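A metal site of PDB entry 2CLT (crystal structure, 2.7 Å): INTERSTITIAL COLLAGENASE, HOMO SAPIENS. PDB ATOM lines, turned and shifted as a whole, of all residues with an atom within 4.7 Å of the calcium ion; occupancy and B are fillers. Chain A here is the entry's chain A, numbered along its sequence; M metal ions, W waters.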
ATOM      1  N   TRP A  10     -16.549  -6.376 -32.286  1.00  0.00           N
ATOM      2  CA  TRP A  10     -16.532  -6.651 -30.836  1.00  0.00           C
ATOM      3  C   TRP A  10     -16.165  -8.118 -30.605  1.00  0.00           C
ATOM      4  O   TRP A  10     -16.691  -9.015 -31.287  1.00  0.00           O
ATOM      5  CB  TRP A  10     -17.901  -6.372 -30.204  1.00  0.00           C
ATOM      6  CG  TRP A  10     -18.314  -4.929 -30.232  1.00  0.00           C
ATOM      7  CD1 TRP A  10     -19.204  -4.348 -31.075  1.00  0.00           C
ATOM      8  CD2 TRP A  10     -17.851  -3.887 -29.363  1.00  0.00           C
ATOM      9  NE1 TRP A  10     -19.332  -3.013 -30.794  1.00  0.00           N
ATOM     10  CE2 TRP A  10     -18.509  -2.705 -29.745  1.00  0.00           C
ATOM     11  CE3 TRP A  10     -16.941  -3.836 -28.293  1.00  0.00           C
ATOM     12  CZ2 TRP A  10     -18.286  -1.477 -29.097  1.00  0.00           C
ATOM     13  CZ3 TRP A  10     -16.724  -2.626 -27.648  1.00  0.00           C
ATOM     14  CH2 TRP A  10     -17.400  -1.456 -28.051  1.00  0.00           C
ATOM     15  N   ALA A  58     -18.890   1.163 -19.795  1.00  0.00           N
ATOM     16  CA  ALA A  58     -19.611   0.164 -20.575  1.00  0.00           C
ATOM     17  C   ALA A  58     -19.030   0.156 -21.986  1.00  0.00           C
ATOM     18  O   ALA A  58     -18.334   1.095 -22.379  1.00  0.00           O
ATOM     19  CB  ALA A  58     -21.101   0.492 -20.605  1.00  0.00           C
ATOM     20  N   ASP A  59     -19.295  -0.904 -22.741  1.00  0.00           N
ATOM     21  CA  ASP A  59     -18.776  -0.985 -24.092  1.00  0.00           C
ATOM     22  C   ASP A  59     -19.281   0.231 -24.848  1.00  0.00           C
ATOM     23  O   ASP A  59     -18.504   0.993 -25.395  1.00  0.00           O
ATOM     24  CB  ASP A  59     -19.255  -2.258 -24.793  1.00  0.00           C
ATOM     25  CG  ASP A  59     -18.886  -3.512 -24.039  1.00  0.00           C
ATOM     26  OD1 ASP A  59     -17.704  -3.674 -23.689  1.00  0.00           O
ATOM     27  OD2 ASP A  59     -19.806  -4.333 -23.789  1.00  0.00           O
ATOM     28  N   ILE A  60     -20.590   0.409 -24.858  1.00  0.00           N
ATOM     29  CA  ILE A  60     -21.183   1.531 -25.566  1.00  0.00           C
ATOM     30  C   ILE A  60     -21.709   2.609 -24.625  1.00  0.00           C
ATOM     31  O   ILE A  60     -22.726   2.435 -23.964  1.00  0.00           O
ATOM     32  CB  ILE A  60     -22.299   1.040 -26.501  1.00  0.00           C
ATOM     33  CG1 ILE A  60     -21.692   0.158 -27.598  1.00  0.00           C
ATOM     34  CG2 ILE A  60     -23.059   2.214 -27.106  1.00  0.00           C
ATOM     35  CD1 ILE A  60     -22.712  -0.663 -28.382  1.00  0.00           C
ATOM     36  N   GLY A  89     -14.365  -1.094 -30.354  1.00  0.00           N
ATOM     37  CA  GLY A  89     -12.991  -1.038 -29.901  1.00  0.00           C
ATOM     38  C   GLY A  89     -12.930  -0.555 -28.488  1.00  0.00           C
ATOM     39  O   GLY A  89     -13.950  -0.208 -27.891  1.00  0.00           O
ATOM     40  N   GLY A  91     -11.861   1.924 -25.154  1.00  0.00           N
ATOM     41  CA  GLY A  91     -12.214   3.306 -24.890  1.00  0.00           C
ATOM     42  C   GLY A  91     -13.432   3.947 -25.523  1.00  0.00           C
ATOM     43  O   GLY A  91     -14.532   3.406 -25.466  1.00  0.00           O
ATOM     44  N   ILE A  92     -13.220   5.121 -26.118  1.00  0.00           N
ATOM     45  CA  ILE A  92     -14.247   5.783 -26.912  1.00  0.00           C
ATOM     46  C   ILE A  92     -14.842   4.893 -28.002  1.00  0.00           C
ATOM     47  O   ILE A  92     -15.815   5.271 -28.645  1.00  0.00           O
ATOM     48  CB  ILE A  92     -13.678   7.075 -27.541  1.00  0.00           C
ATOM     49  CG1 ILE A  92     -14.789   8.130 -27.670  1.00  0.00           C
ATOM     50  CG2 ILE A  92     -13.061   6.781 -28.901  1.00  0.00           C
ATOM     51  CD1 ILE A  92     -14.400   9.321 -28.513  1.00  0.00           C
ATOM     52  N   GLY A  93     -14.256   3.711 -28.209  1.00  0.00           N
ATOM     53  CA  GLY A  93     -14.810   2.805 -29.209  1.00  0.00           C
ATOM     54  C   GLY A  93     -16.252   2.407 -28.964  1.00  0.00           C
ATOM     55  O   GLY A  93     -16.645   2.137 -27.851  1.00  0.00           O
ATOM     56  N   GLY A  94     -17.046   2.379 -30.030  1.00  0.00           N
ATOM     57  CA  GLY A  94     -18.440   2.000 -29.885  1.00  0.00           C
ATOM     58  C   GLY A  94     -19.360   3.061 -29.306  1.00  0.00           C
ATOM     59  O   GLY A  94     -20.572   2.885 -29.298  1.00  0.00           O
ATOM     60  N   ASP A  95     -18.797   4.178 -28.838  1.00  0.00           N
ATOM     61  CA  ASP A  95     -19.633   5.220 -28.249  1.00  0.00           C
ATOM     62  C   ASP A  95     -20.401   6.021 -29.285  1.00  0.00           C
ATOM     63  O   ASP A  95     -19.940   6.215 -30.405  1.00  0.00           O
ATOM     64  CB  ASP A  95     -18.796   6.155 -27.373  1.00  0.00           C
ATOM     65  CG  ASP A  95     -18.145   5.427 -26.197  1.00  0.00           C
ATOM     66  OD1 ASP A  95     -18.125   5.998 -25.090  1.00  0.00           O
ATOM     67  OD2 ASP A  95     -17.630   4.299 -26.386  1.00  0.00           O
HETATM   68 CA    CA M   1     -16.544   2.358 -25.811  1.00  0.00          CA
HETATM   69  O   HOH W   1     -15.185   0.419 -25.296  1.00  0.00           O
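O of Gly 93 is bound to the calcium ion (2.1 Å). O of Gly 91 is bound to the calcium ion. The calcium ion is bound by OD2 of Asp 95 (2.3 Å). Water W1 binds the calcium ion. O of Asp 59 is bound to the calcium ion, at 2.4 Å. The calcium ion has five donor atoms within binding distance.
Ile 92 touches the calcium ion (C to CA, 3.8 Å). Of the 10 residues printed, 5 come within 4 Å of the calcium ion.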
